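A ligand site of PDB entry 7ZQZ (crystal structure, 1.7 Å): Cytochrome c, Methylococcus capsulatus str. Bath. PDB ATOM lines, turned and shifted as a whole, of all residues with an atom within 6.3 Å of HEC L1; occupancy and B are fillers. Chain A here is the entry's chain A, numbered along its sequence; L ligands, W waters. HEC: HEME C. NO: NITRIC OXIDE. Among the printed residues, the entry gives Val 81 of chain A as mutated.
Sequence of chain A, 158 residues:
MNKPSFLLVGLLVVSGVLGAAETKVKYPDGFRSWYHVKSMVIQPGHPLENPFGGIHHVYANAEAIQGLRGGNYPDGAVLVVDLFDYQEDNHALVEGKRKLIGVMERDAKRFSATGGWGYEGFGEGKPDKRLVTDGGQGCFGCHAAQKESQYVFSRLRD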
ATOM      1  N   LYS A  38     -26.891   3.862 -37.482  1.00  0.00           N
ATOM      2  CA  LYS A  38     -26.574   2.446 -37.233  1.00  0.00           C
ATOM      3  C   LYS A  38     -27.006   2.097 -35.803  1.00  0.00           C
ATOM      4  O   LYS A  38     -27.349   3.036 -35.015  1.00  0.00           O
ATOM      5  CB  LYS A  38     -25.060   2.222 -37.317  1.00  0.00           C
ATOM      6  CG  LYS A  38     -24.216   2.854 -36.219  1.00  0.00           C
ATOM      7  CD  LYS A  38     -22.794   2.451 -36.206  1.00  0.00           C
ATOM      8  CE  LYS A  38     -22.619   0.989 -35.877  1.00  0.00           C
ATOM      9  NZ  LYS A  38     -21.184   0.727 -35.742  1.00  0.00           N
ATOM     10  N   SER A  39     -26.935   0.817 -35.490  1.00  0.00           N
ATOM     11  CA  SER A  39     -27.254   0.265 -34.153  1.00  0.00           C
ATOM     12  C   SER A  39     -26.226  -0.805 -33.837  1.00  0.00           C
ATOM     13  O   SER A  39     -25.603  -1.370 -34.771  1.00  0.00           O
ATOM     14  CB  SER A  39     -28.632  -0.274 -34.057  1.00  0.00           C
ATOM     15  OG  SER A  39     -29.624   0.668 -34.405  1.00  0.00           O
ATOM     16  N   MET A  40     -26.126  -1.143 -32.544  1.00  0.00           N
ATOM     17  CA  MET A  40     -25.242  -2.234 -32.082  1.00  0.00           C
ATOM     18  C   MET A  40     -25.805  -2.709 -30.717  1.00  0.00           C
ATOM     19  O   MET A  40     -26.505  -1.890 -30.053  1.00  0.00           O
ATOM     20  CB  MET A  40     -23.805  -1.744 -31.948  1.00  0.00           C
ATOM     21  CG  MET A  40     -22.788  -2.785 -31.490  1.00  0.00           C
ATOM     22  SD  MET A  40     -21.198  -2.049 -31.172  1.00  0.00           S
ATOM     23  CE  MET A  40     -20.619  -1.810 -32.854  1.00  0.00           C
ATOM     24  N   ILE A  42     -24.564  -4.408 -27.030  1.00  0.00           N
ATOM     25  CA  ILE A  42     -23.446  -4.726 -26.103  1.00  0.00           C
ATOM     26  C   ILE A  42     -24.045  -5.563 -24.957  1.00  0.00           C
ATOM     27  O   ILE A  42     -25.057  -5.104 -24.323  1.00  0.00           O
ATOM     28  CB  ILE A  42     -22.739  -3.461 -25.624  1.00  0.00           C
ATOM     29  CG1 ILE A  42     -22.041  -2.789 -26.835  1.00  0.00           C
ATOM     30  CG2 ILE A  42     -21.758  -3.786 -24.489  1.00  0.00           C
ATOM     31  CD1 ILE A  42     -21.363  -1.498 -26.554  1.00  0.00           C
ATOM     32  N   LEU A  48     -17.039  -3.096 -22.283  1.00  0.00           N
ATOM     33  CA  LEU A  48     -17.749  -1.784 -22.140  1.00  0.00           C
ATOM     34  C   LEU A  48     -19.146  -1.968 -21.486  1.00  0.00           C
ATOM     35  O   LEU A  48     -19.948  -0.996 -21.470  1.00  0.00           O
ATOM     36  CB  LEU A  48     -17.867  -1.146 -23.539  1.00  0.00           C
ATOM     37  CG  LEU A  48     -16.543  -0.826 -24.254  1.00  0.00           C
ATOM     38  CD1 LEU A  48     -16.791  -0.057 -25.551  1.00  0.00           C
ATOM     39  CD2 LEU A  48     -15.576  -0.067 -23.361  1.00  0.00           C
ATOM     40  N   PHE A  52     -22.022   0.918 -20.952  1.00  0.00           N
ATOM     41  CA  PHE A  52     -22.524   0.974 -22.358  1.00  0.00           C
ATOM     42  C   PHE A  52     -23.367  -0.229 -22.729  1.00  0.00           C
ATOM     43  O   PHE A  52     -23.847  -0.316 -23.859  1.00  0.00           O
ATOM     44  CB  PHE A  52     -21.345   1.184 -23.321  1.00  0.00           C
ATOM     45  CG  PHE A  52     -21.648   1.808 -24.676  1.00  0.00           C
ATOM     46  CD1 PHE A  52     -22.793   2.541 -24.922  1.00  0.00           C
ATOM     47  CD2 PHE A  52     -20.695   1.771 -25.687  1.00  0.00           C
ATOM     48  CE1 PHE A  52     -23.030   3.136 -26.163  1.00  0.00           C
ATOM     49  CE2 PHE A  52     -20.895   2.404 -26.905  1.00  0.00           C
ATOM     50  CZ  PHE A  52     -22.075   3.075 -27.135  1.00  0.00           C
ATOM     51  N   HIS A  56     -28.005   0.155 -28.576  1.00  0.00           N
ATOM     52  CA  HIS A  56     -27.817   1.595 -28.879  1.00  0.00           C
ATOM     53  C   HIS A  56     -28.035   1.908 -30.359  1.00  0.00           C
ATOM     54  O   HIS A  56     -27.785   1.055 -31.206  1.00  0.00           O
ATOM     55  CB  HIS A  56     -26.523   2.112 -28.344  1.00  0.00           C
ATOM     56  CG  HIS A  56     -25.304   1.702 -29.088  1.00  0.00           C
ATOM     57  ND1 HIS A  56     -24.435   0.815 -28.553  1.00  0.00           N
ATOM     58  CD2 HIS A  56     -24.748   2.158 -30.233  1.00  0.00           C
ATOM     59  CE1 HIS A  56     -23.368   0.681 -29.365  1.00  0.00           C
ATOM     60  NE2 HIS A  56     -23.566   1.491 -30.422  1.00  0.00           N
ATOM     61  N   VAL A  58     -27.423   5.143 -33.196  1.00  0.00           N
ATOM     62  CA  VAL A  58     -26.699   6.389 -33.466  1.00  0.00           C
ATOM     63  C   VAL A  58     -27.543   7.240 -34.410  1.00  0.00           C
ATOM     64  O   VAL A  58     -28.069   6.711 -35.417  1.00  0.00           O
ATOM     65  CB  VAL A  58     -25.305   6.115 -34.031  1.00  0.00           C
ATOM     66  CG1 VAL A  58     -24.520   7.394 -34.339  1.00  0.00           C
ATOM     67  CG2 VAL A  58     -24.489   5.216 -33.115  1.00  0.00           C
ATOM     68  N   LEU A  79     -23.907  14.355 -33.213  1.00  0.00           N
ATOM     69  CA  LEU A  79     -24.140  12.897 -33.170  1.00  0.00           C
ATOM     70  C   LEU A  79     -24.713  12.562 -31.790  1.00  0.00           C
ATOM     71  O   LEU A  79     -24.184  13.090 -30.774  1.00  0.00           O
ATOM     72  CB  LEU A  79     -22.806  12.184 -33.408  1.00  0.00           C
ATOM     73  CG  LEU A  79     -22.278  12.373 -34.848  1.00  0.00           C
ATOM     74  CD1 LEU A  79     -20.794  12.106 -34.896  1.00  0.00           C
ATOM     75  CD2 LEU A  79     -23.062  11.486 -35.766  1.00  0.00           C
ATOM     76  N   VAL A  80     -25.681  11.658 -31.785  1.00  0.00           N
ATOM     77  CA  VAL A  80     -26.301  11.154 -30.542  1.00  0.00           C
ATOM     78  C   VAL A  80     -26.227   9.647 -30.521  1.00  0.00           C
ATOM     79  O   VAL A  80     -26.592   9.018 -31.521  1.00  0.00           O
ATOM     80  CB  VAL A  80     -27.739  11.621 -30.356  1.00  0.00           C
ATOM     81  CG1 VAL A  80     -28.343  11.169 -29.019  1.00  0.00           C
ATOM     82  CG2 VAL A  80     -27.822  13.119 -30.510  1.00  0.00           C
ATOM     83  N   VAL A  81     -25.745   9.113 -29.401  1.00  0.00           N
ATOM     84  CA  VAL A  81     -25.891   7.652 -29.205  1.00  0.00           C
ATOM     85  C   VAL A  81     -26.961   7.432 -28.118  1.00  0.00           C
ATOM     86  O   VAL A  81     -26.843   8.032 -27.005  1.00  0.00           O
ATOM     87  CB  VAL A  81     -24.542   6.965 -28.902  1.00  0.00           C
ATOM     88  CG1 VAL A  81     -23.853   7.494 -27.661  1.00  0.00           C
ATOM     89  CG2 VAL A  81     -24.762   5.470 -28.782  1.00  0.00           C
ATOM     90  N   ILE A 101     -28.377   9.050 -23.058  1.00  0.00           N
ATOM     91  CA  ILE A 101     -27.818   9.390 -24.380  1.00  0.00           C
ATOM     92  C   ILE A 101     -26.418   9.966 -24.186  1.00  0.00           C
ATOM     93  O   ILE A 101     -26.117  10.623 -23.154  1.00  0.00           O
ATOM     94  CB  ILE A 101     -28.740  10.308 -25.160  1.00  0.00           C
ATOM     95  CG1 ILE A 101     -28.716  11.737 -24.609  1.00  0.00           C
ATOM     96  CG2 ILE A 101     -30.124   9.715 -25.266  1.00  0.00           C
ATOM     97  CD1 ILE A 101     -29.572  12.734 -25.370  1.00  0.00           C
ATOM     98  N   GLY A 102     -25.553   9.705 -25.158  1.00  0.00           N
ATOM     99  CA  GLY A 102     -24.268  10.390 -25.308  1.00  0.00           C
ATOM    100  C   GLY A 102     -24.341  11.351 -26.494  1.00  0.00           C
ATOM    101  O   GLY A 102     -25.038  11.042 -27.494  1.00  0.00           O
ATOM    102  N   VAL A 103     -23.709  12.505 -26.378  1.00  0.00           N
ATOM    103  CA  VAL A 103     -23.852  13.580 -27.367  1.00  0.00           C
ATOM    104  C   VAL A 103     -22.473  14.140 -27.702  1.00  0.00           C
ATOM    105  O   VAL A 103     -21.663  14.454 -26.777  1.00  0.00           O
ATOM    106  CB  VAL A 103     -24.819  14.677 -26.914  1.00  0.00           C
ATOM    107  CG1 VAL A 103     -24.962  15.748 -27.976  1.00  0.00           C
ATOM    108  CG2 VAL A 103     -26.162  14.101 -26.496  1.00  0.00           C
ATOM    109  N   MET A 104     -22.216  14.297 -29.001  1.00  0.00           N
ATOM    110  CA  MET A 104     -21.008  15.002 -29.514  1.00  0.00           C
ATOM    111  C   MET A 104     -21.477  16.196 -30.363  1.00  0.00           C
ATOM    112  O   MET A 104     -22.265  15.991 -31.276  1.00  0.00           O
ATOM    113  CB  MET A 104     -20.185  14.062 -30.403  1.00  0.00           C
ATOM    114  CG  MET A 104     -19.472  13.035 -29.634  1.00  0.00           C
ATOM    115  SD  MET A 104     -18.786  11.688 -30.704  1.00  0.00           S
ATOM    116  CE  MET A 104     -17.474  12.534 -31.592  1.00  0.00           C
ATOM    117  N   GLY A 118     -17.544  18.658 -28.478  1.00  0.00           N
ATOM    118  CA  GLY A 118     -17.952  18.723 -27.073  1.00  0.00           C
ATOM    119  C   GLY A 118     -18.695  17.450 -26.726  1.00  0.00           C
ATOM    120  O   GLY A 118     -19.588  17.044 -27.518  1.00  0.00           O
ATOM    121  N   TYR A 119     -18.378  16.825 -25.605  1.00  0.00           N
ATOM    122  CA  TYR A 119     -18.892  15.525 -25.161  1.00  0.00           C
ATOM    123  C   TYR A 119     -19.789  15.732 -23.913  1.00  0.00           C
ATOM    124  O   TYR A 119     -19.347  16.344 -22.937  1.00  0.00           O
ATOM    125  CB  TYR A 119     -17.750  14.574 -24.838  1.00  0.00           C
ATOM    126  CG  TYR A 119     -16.910  14.130 -26.016  1.00  0.00           C
ATOM    127  CD1 TYR A 119     -15.813  14.867 -26.441  1.00  0.00           C
ATOM    128  CD2 TYR A 119     -17.220  12.975 -26.731  1.00  0.00           C
ATOM    129  CE1 TYR A 119     -15.039  14.465 -27.522  1.00  0.00           C
ATOM    130  CE2 TYR A 119     -16.438  12.550 -27.786  1.00  0.00           C
ATOM    131  CZ  TYR A 119     -15.344  13.296 -28.187  1.00  0.00           C
ATOM    132  OH  TYR A 119     -14.630  12.896 -29.293  1.00  0.00           O
ATOM    133  N   GLU A 120     -21.027  15.213 -23.941  1.00  0.00           N
ATOM    134  CA  GLU A 120     -21.943  15.287 -22.771  1.00  0.00           C
ATOM    135  C   GLU A 120     -22.773  14.021 -22.753  1.00  0.00           C
ATOM    136  O   GLU A 120     -23.050  13.449 -23.838  1.00  0.00           O
ATOM    137  CB  GLU A 120     -22.787  16.550 -22.874  1.00  0.00           C
ATOM    138  CG  GLU A 120     -23.810  16.627 -21.745  1.00  0.00           C
ATOM    139  CD  GLU A 120     -23.121  16.839 -20.426  1.00  0.00           C
ATOM    140  OE1 GLU A 120     -23.046  18.028 -20.005  1.00  0.00           O
ATOM    141  OE2 GLU A 120     -22.699  15.859 -19.859  1.00  0.00           O
ATOM    142  N   GLY A 121     -23.160  13.612 -21.561  1.00  0.00           N
ATOM    143  CA  GLY A 121     -24.099  12.522 -21.370  1.00  0.00           C
ATOM    144  C   GLY A 121     -25.349  13.071 -20.721  1.00  0.00           C
ATOM    145  O   GLY A 121     -25.213  13.964 -19.871  1.00  0.00           O
ATOM    146  N   LEU A 131     -24.166  14.387 -17.228  1.00  0.00           N
ATOM    147  CA  LEU A 131     -23.323  13.370 -16.580  1.00  0.00           C
ATOM    148  C   LEU A 131     -21.858  13.748 -16.536  1.00  0.00           C
ATOM    149  O   LEU A 131     -21.162  13.235 -15.677  1.00  0.00           O
ATOM    150  CB  LEU A 131     -23.532  12.044 -17.287  1.00  0.00           C
ATOM    151  CG  LEU A 131     -24.960  11.523 -17.290  1.00  0.00           C
ATOM    152  CD1 LEU A 131     -25.001  10.265 -18.094  1.00  0.00           C
ATOM    153  CD2 LEU A 131     -25.499  11.277 -15.893  1.00  0.00           C
ATOM    154  N   VAL A 132     -21.373  14.510 -17.509  1.00  0.00           N
ATOM    155  CA  VAL A 132     -19.902  14.704 -17.671  1.00  0.00           C
ATOM    156  C   VAL A 132     -19.416  15.744 -16.652  1.00  0.00           C
ATOM    157  O   VAL A 132     -20.017  16.809 -16.551  1.00  0.00           O
ATOM    158  CB  VAL A 132     -19.545  15.104 -19.106  1.00  0.00           C
ATOM    159  CG1 VAL A 132     -18.132  15.655 -19.221  1.00  0.00           C
ATOM    160  CG2 VAL A 132     -19.740  13.897 -20.037  1.00  0.00           C
ATOM    161  N   GLY A 136     -15.273  16.482 -20.490  1.00  0.00           N
ATOM    162  CA  GLY A 136     -15.372  15.478 -21.570  1.00  0.00           C
ATOM    163  C   GLY A 136     -14.006  14.850 -21.873  1.00  0.00           C
ATOM    164  O   GLY A 136     -13.922  14.171 -22.876  1.00  0.00           O
ATOM    165  N   GLY A 138     -12.518  12.265 -20.344  1.00  0.00           N
ATOM    166  CA  GLY A 138     -12.731  10.800 -20.338  1.00  0.00           C
ATOM    167  C   GLY A 138     -13.339  10.307 -21.653  1.00  0.00           C
ATOM    168  O   GLY A 138     -12.855   9.322 -22.246  1.00  0.00           O
ATOM    169  N   CYS A 139     -14.418  10.926 -22.106  1.00  0.00           N
ATOM    170  CA  CYS A 139     -15.033  10.572 -23.396  1.00  0.00           C
ATOM    171  C   CYS A 139     -13.966  10.693 -24.501  1.00  0.00           C
ATOM    172  O   CYS A 139     -13.815   9.759 -25.336  1.00  0.00           O
ATOM    173  CB  CYS A 139     -16.224  11.474 -23.750  1.00  0.00           C
ATOM    174  SG  CYS A 139     -17.480  11.687 -22.446  1.00  0.00           S
ATOM    175  N   PHE A 140     -13.340  11.863 -24.581  1.00  0.00           N
ATOM    176  CA  PHE A 140     -12.365  12.194 -25.662  1.00  0.00           C
ATOM    177  C   PHE A 140     -11.254  11.140 -25.663  1.00  0.00           C
ATOM    178  O   PHE A 140     -10.784  10.768 -26.745  1.00  0.00           O
ATOM    179  CB  PHE A 140     -11.821  13.600 -25.437  1.00  0.00           C
ATOM    180  CG  PHE A 140     -10.757  14.002 -26.423  1.00  0.00           C
ATOM    181  CD1 PHE A 140     -10.992  13.934 -27.782  1.00  0.00           C
ATOM    182  CD2 PHE A 140      -9.529  14.477 -25.976  1.00  0.00           C
ATOM    183  CE1 PHE A 140     -10.019  14.330 -28.690  1.00  0.00           C
ATOM    184  CE2 PHE A 140      -8.557  14.883 -26.883  1.00  0.00           C
ATOM    185  CZ  PHE A 140      -8.811  14.804 -28.237  1.00  0.00           C
ATOM    186  N   GLY A 141     -10.838  10.660 -24.477  1.00  0.00           N
ATOM    187  CA  GLY A 141      -9.699   9.746 -24.338  1.00  0.00           C
ATOM    188  C   GLY A 141      -9.949   8.429 -25.042  1.00  0.00           C
ATOM    189  O   GLY A 141      -8.995   7.860 -25.564  1.00  0.00           O
ATOM    190  N   CYS A 142     -11.195   7.972 -25.095  1.00  0.00           N
ATOM    191  CA  CYS A 142     -11.549   6.738 -25.824  1.00  0.00           C
ATOM    192  C   CYS A 142     -11.716   7.092 -27.305  1.00  0.00           C
ATOM    193  O   CYS A 142     -11.276   6.290 -28.173  1.00  0.00           O
ATOM    194  CB  CYS A 142     -12.790   6.078 -25.245  1.00  0.00           C
ATOM    195  SG  CYS A 142     -13.151   4.465 -25.994  1.00  0.00           S
ATOM    196  N   HIS A 143     -12.358   8.221 -27.616  1.00  0.00           N
ATOM    197  CA  HIS A 143     -12.580   8.620 -29.035  1.00  0.00           C
ATOM    198  C   HIS A 143     -11.235   8.976 -29.711  1.00  0.00           C
ATOM    199  O   HIS A 143     -11.218   9.048 -30.946  1.00  0.00           O
ATOM    200  CB  HIS A 143     -13.573   9.774 -29.155  1.00  0.00           C
ATOM    201  CG  HIS A 143     -14.982   9.348 -28.979  1.00  0.00           C
ATOM    202  ND1 HIS A 143     -15.850   9.275 -30.044  1.00  0.00           N
ATOM    203  CD2 HIS A 143     -15.698   8.985 -27.873  1.00  0.00           C
ATOM    204  CE1 HIS A 143     -17.032   8.838 -29.601  1.00  0.00           C
ATOM    205  NE2 HIS A 143     -16.951   8.629 -28.292  1.00  0.00           N
ATOM    206  N   TYR A 151     -12.606  11.525 -34.923  1.00  0.00           N
ATOM    207  CA  TYR A 151     -12.914  11.079 -33.538  1.00  0.00           C
ATOM    208  C   TYR A 151     -14.284  10.414 -33.497  1.00  0.00           C
ATOM    209  O   TYR A 151     -14.780  10.138 -32.345  1.00  0.00           O
ATOM    210  CB  TYR A 151     -12.866  12.254 -32.575  1.00  0.00           C
ATOM    211  CG  TYR A 151     -11.517  12.924 -32.546  1.00  0.00           C
ATOM    212  CD1 TYR A 151     -10.456  12.272 -31.944  1.00  0.00           C
ATOM    213  CD2 TYR A 151     -11.278  14.131 -33.188  1.00  0.00           C
ATOM    214  CE1 TYR A 151      -9.191  12.849 -31.887  1.00  0.00           C
ATOM    215  CE2 TYR A 151     -10.016  14.718 -33.140  1.00  0.00           C
ATOM    216  CZ  TYR A 151      -8.981  14.072 -32.487  1.00  0.00           C
ATOM    217  OH  TYR A 151      -7.717  14.587 -32.404  1.00  0.00           O
ATOM    218  N   VAL A 152     -14.830  10.079 -34.660  1.00  0.00           N
ATOM    219  CA  VAL A 152     -16.138   9.398 -34.796  1.00  0.00           C
ATOM    220  C   VAL A 152     -15.926   7.899 -35.119  1.00  0.00           C
ATOM    221  O   VAL A 152     -15.252   7.582 -36.143  1.00  0.00           O
ATOM    222  CB  VAL A 152     -16.987  10.079 -35.878  1.00  0.00           C
ATOM    223  CG1 VAL A 152     -18.267   9.305 -36.104  1.00  0.00           C
ATOM    224  CG2 VAL A 152     -17.261  11.551 -35.590  1.00  0.00           C
ATOM    225  N   PHE A 153     -16.479   7.010 -34.316  1.00  0.00           N
ATOM    226  CA  PHE A 153     -16.453   5.545 -34.560  1.00  0.00           C
ATOM    227  C   PHE A 153     -17.403   5.136 -35.681  1.00  0.00           C
ATOM    228  O   PHE A 153     -17.057   4.220 -36.489  1.00  0.00           O
ATOM    229  CB  PHE A 153     -16.874   4.702 -33.341  1.00  0.00           C
ATOM    230  CG  PHE A 153     -15.943   4.745 -32.171  1.00  0.00           C
ATOM    231  CD1 PHE A 153     -16.092   5.728 -31.187  1.00  0.00           C
ATOM    232  CD2 PHE A 153     -14.941   3.791 -32.037  1.00  0.00           C
ATOM    233  CE1 PHE A 153     -15.225   5.767 -30.092  1.00  0.00           C
ATOM    234  CE2 PHE A 153     -14.100   3.819 -30.925  1.00  0.00           C
ATOM    235  CZ  PHE A 153     -14.223   4.813 -29.958  1.00  0.00           C
ATOM    236  N   SER A 154     -18.639   5.626 -35.658  1.00  0.00           N
ATOM    237  CA  SER A 154     -19.717   5.116 -36.519  1.00  0.00           C
ATOM    238  C   SER A 154     -19.366   5.387 -37.984  1.00  0.00           C
ATOM    239  O   SER A 154     -18.886   6.535 -38.273  1.00  0.00           O
ATOM    240  CB  SER A 154     -21.061   5.763 -36.210  1.00  0.00           C
ATOM    241  OG  SER A 154     -21.526   5.426 -34.926  1.00  0.00           O
ATOM    242  N   ARG A 155     -19.673   4.426 -38.851  1.00  0.00           N
ATOM    243  CA  ARG A 155     -19.588   4.559 -40.342  1.00  0.00           C
ATOM    244  C   ARG A 155     -21.005   4.558 -40.934  1.00  0.00           C
ATOM    245  O   ARG A 155     -21.854   3.737 -40.591  1.00  0.00           O
ATOM    246  CB  ARG A 155     -18.777   3.417 -40.972  1.00  0.00           C
ATOM    247  CG  ARG A 155     -17.370   3.272 -40.431  1.00  0.00           C
ATOM    248  CD  ARG A 155     -16.435   4.438 -40.699  1.00  0.00           C
ATOM    249  NE  ARG A 155     -15.170   4.170 -40.010  1.00  0.00           N
ATOM    250  CZ  ARG A 155     -14.736   4.769 -38.886  1.00  0.00           C
ATOM    251  NH1 ARG A 155     -15.395   5.789 -38.353  1.00  0.00           N
ATOM    252  NH2 ARG A 155     -13.619   4.391 -38.320  1.00  0.00           N
HETATM  253 FE   HEC L   1     -18.809   6.821 -26.933  1.00  0.00          FE
HETATM  254  CHA HEC L   1     -20.068   5.992 -30.007  1.00  0.00           C
HETATM  255  CHB HEC L   1     -20.512   9.811 -27.045  1.00  0.00           C
HETATM  256  CHC HEC L   1     -17.434   7.718 -23.951  1.00  0.00           C
HETATM  257  CHD HEC L   1     -16.752   4.114 -27.081  1.00  0.00           C
HETATM  258  NA  HEC L   1     -20.009   7.711 -28.228  1.00  0.00           N
HETATM  259  C1A HEC L   1     -20.387   7.205 -29.507  1.00  0.00           C
HETATM  260  C2A HEC L   1     -21.202   8.192 -30.166  1.00  0.00           C
HETATM  261  C3A HEC L   1     -21.333   9.247 -29.327  1.00  0.00           C
HETATM  262  C4A HEC L   1     -20.600   8.968 -28.146  1.00  0.00           C
HETATM  263  CMA HEC L   1     -22.115  10.534 -29.605  1.00  0.00           C
HETATM  264  CAA HEC L   1     -21.736   8.029 -31.590  1.00  0.00           C
HETATM  265  CBA HEC L   1     -20.766   8.724 -32.587  1.00  0.00           C
HETATM  266  CGA HEC L   1     -19.536   7.842 -32.840  1.00  0.00           C
HETATM  267  O1A HEC L   1     -19.670   6.713 -33.385  1.00  0.00           O
HETATM  268  O2A HEC L   1     -18.410   8.234 -32.495  1.00  0.00           O
HETATM  269  NB  HEC L   1     -18.941   8.497 -25.728  1.00  0.00           N
HETATM  270  C1B HEC L   1     -19.732   9.559 -25.948  1.00  0.00           C
HETATM  271  C2B HEC L   1     -19.630  10.427 -24.797  1.00  0.00           C
HETATM  272  C3B HEC L   1     -18.769   9.839 -23.878  1.00  0.00           C
HETATM  273  C4B HEC L   1     -18.352   8.590 -24.546  1.00  0.00           C
HETATM  274  CMB HEC L   1     -20.431  11.710 -24.650  1.00  0.00           C
HETATM  275  CAB HEC L   1     -18.339  10.222 -22.436  1.00  0.00           C
HETATM  276  CBB HEC L   1     -19.426  10.478 -21.650  1.00  0.00           C
HETATM  277  NC  HEC L   1     -17.366   6.038 -25.723  1.00  0.00           N
HETATM  278  C1C HEC L   1     -16.915   6.593 -24.545  1.00  0.00           C
HETATM  279  C2C HEC L   1     -15.767   5.852 -24.080  1.00  0.00           C
HETATM  280  C3C HEC L   1     -15.523   4.794 -24.995  1.00  0.00           C
HETATM  281  C4C HEC L   1     -16.576   4.947 -25.997  1.00  0.00           C
HETATM  282  CMC HEC L   1     -15.051   6.227 -22.798  1.00  0.00           C
HETATM  283  CAC HEC L   1     -14.443   3.703 -25.031  1.00  0.00           C
HETATM  284  CBC HEC L   1     -13.771   3.417 -23.884  1.00  0.00           C
HETATM  285  ND  HEC L   1     -18.510   5.392 -28.219  1.00  0.00           N
HETATM  286  C1D HEC L   1     -17.624   4.358 -28.098  1.00  0.00           C
HETATM  287  C2D HEC L   1     -17.756   3.397 -29.217  1.00  0.00           C
HETATM  288  C3D HEC L   1     -18.722   3.927 -30.036  1.00  0.00           C
HETATM  289  C4D HEC L   1     -19.175   5.178 -29.388  1.00  0.00           C
HETATM  290  CMD HEC L   1     -16.940   2.120 -29.420  1.00  0.00           C
HETATM  291  CAD HEC L   1     -19.201   3.343 -31.344  1.00  0.00           C
HETATM  292  CBD HEC L   1     -20.447   2.481 -31.116  1.00  0.00           C
HETATM  293  CGD HEC L   1     -20.959   1.855 -32.397  1.00  0.00           C
HETATM  294  O1D HEC L   1     -22.147   1.517 -32.561  1.00  0.00           O
HETATM  295  O2D HEC L   1     -20.146   1.756 -33.392  1.00  0.00           O
HETATM  296  N    NO L   2     -20.313   5.997 -26.195  1.00  0.00           N
HETATM  297  O    NO L   2     -21.354   6.521 -25.725  1.00  0.00           O
HETATM  298  O   HOH W   1     -17.526   0.865 -33.778  1.00  0.00           O
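The side-chain sulfur of Cys 139 is bonded to a carbon (CAB) of HEC L1, at 1.7 Å. SG of Cys 142 is covalently linked to CAC of HEC L1 (1.8 Å). A ring nitrogen (NE2) of His 56 is in hydrogen-bond range of an oxygen (O1D) of HEC L1 (2.6 Å). O1A of HEC L1 lies within hydrogen-bond range of N of Ser 154 (2.7 Å). OG of Ser 154 lies within hydrogen-bond range of O1A of HEC L1 (2.7 Å). NZ of Lys 38 is in salt-bridge range of O2D of HEC L1 (2.8 Å). N of Phe 153 lies within hydrogen-bond range of O2A of HEC L1 (2.9 Å).
A nitrogen (N) of NO L2 is bound to an iron atom (FE) of HEC L1 (1.9 Å).
The backbone NH (N) of His 56 sits at hydrogen-bond distance from the backbone carbonyl oxygen (O) of Met 40 (2.9 Å). N of Val 58 sits at hydrogen-bond distance from O of Lys 38, at 2.8 Å. NH1 of Arg 155 is in hydrogen-bond range of O of Phe 153 (2.9 Å). O of Tyr 151 sits at hydrogen-bond distance from ND1 of His 143 (2.7 Å). The backbone NH of Val 103 lies within hydrogen-bond range of the backbone carbonyl oxygen of Glu 120, 2.8 Å away. The guanidinium group of Arg 155 is in hydrogen-bond range of the backbone carbonyl oxygen of Val 152 (2.8 Å). The backbone carbonyl oxygen (O) of Leu 79 is in hydrogen-bond range of the backbone NH (N) of Met 104, at 2.9 Å. The backbone NH (N) of Val 81 is in hydrogen-bond range of the backbone carbonyl oxygen (O) of Gly 102.
NE2 of His 143 sits close to NA of HEC L1 (3.2 Å). CE of Met 40 touches O2D of HEC L1, at 3.6 Å. Leu 48 touches HEC L1 (CD2 to CBC, 3.96 Å). Phe 52 touches HEC L1 (CE2 to C1D, 3.99 Å). CG1 of Val 58 touches CAA of HEC L1, at 3.96 Å. Leu 79 touches HEC L1. Val 81 touches HEC L1 (CG1 to C3A, 3.5 Å). Gly 102 touches HEC L1 (O to CMA, 3.6 Å). O of Val 103 touches CMB of HEC L1, at 3.7 Å. Met 104 touches HEC L1. Tyr 119 touches HEC L1. Glu 120 touches HEC L1 (O to CMB, 3.2 Å). Val 132 touches HEC L1. O of Gly 138 touches CMC of HEC L1, 3.8 Å away. Val 152 touches HEC L1. Hydrophobic or aromatic side chains within 4 Å of HEC L1: Met 40, Leu 48, Phe 52, His 56, Val 58, Val 81, Met 104, Tyr 119, Val 132, His 143, Val 152 and Phe 153. Within 4 Å of HEC L1: Lys 38, Met 40, Leu 48, Phe 52, His 56, Val 58, Leu 79, Val 81, Gly 102, Val 103, Met 104, Tyr 119, Glu 120, Val 132, Gly 138, Cys 139, Cys 142, His 143, Val 152, Phe 153 and Ser 154. The nearest printed residue that does not touch HEC L1 is Tyr 151 (4.1 Å).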
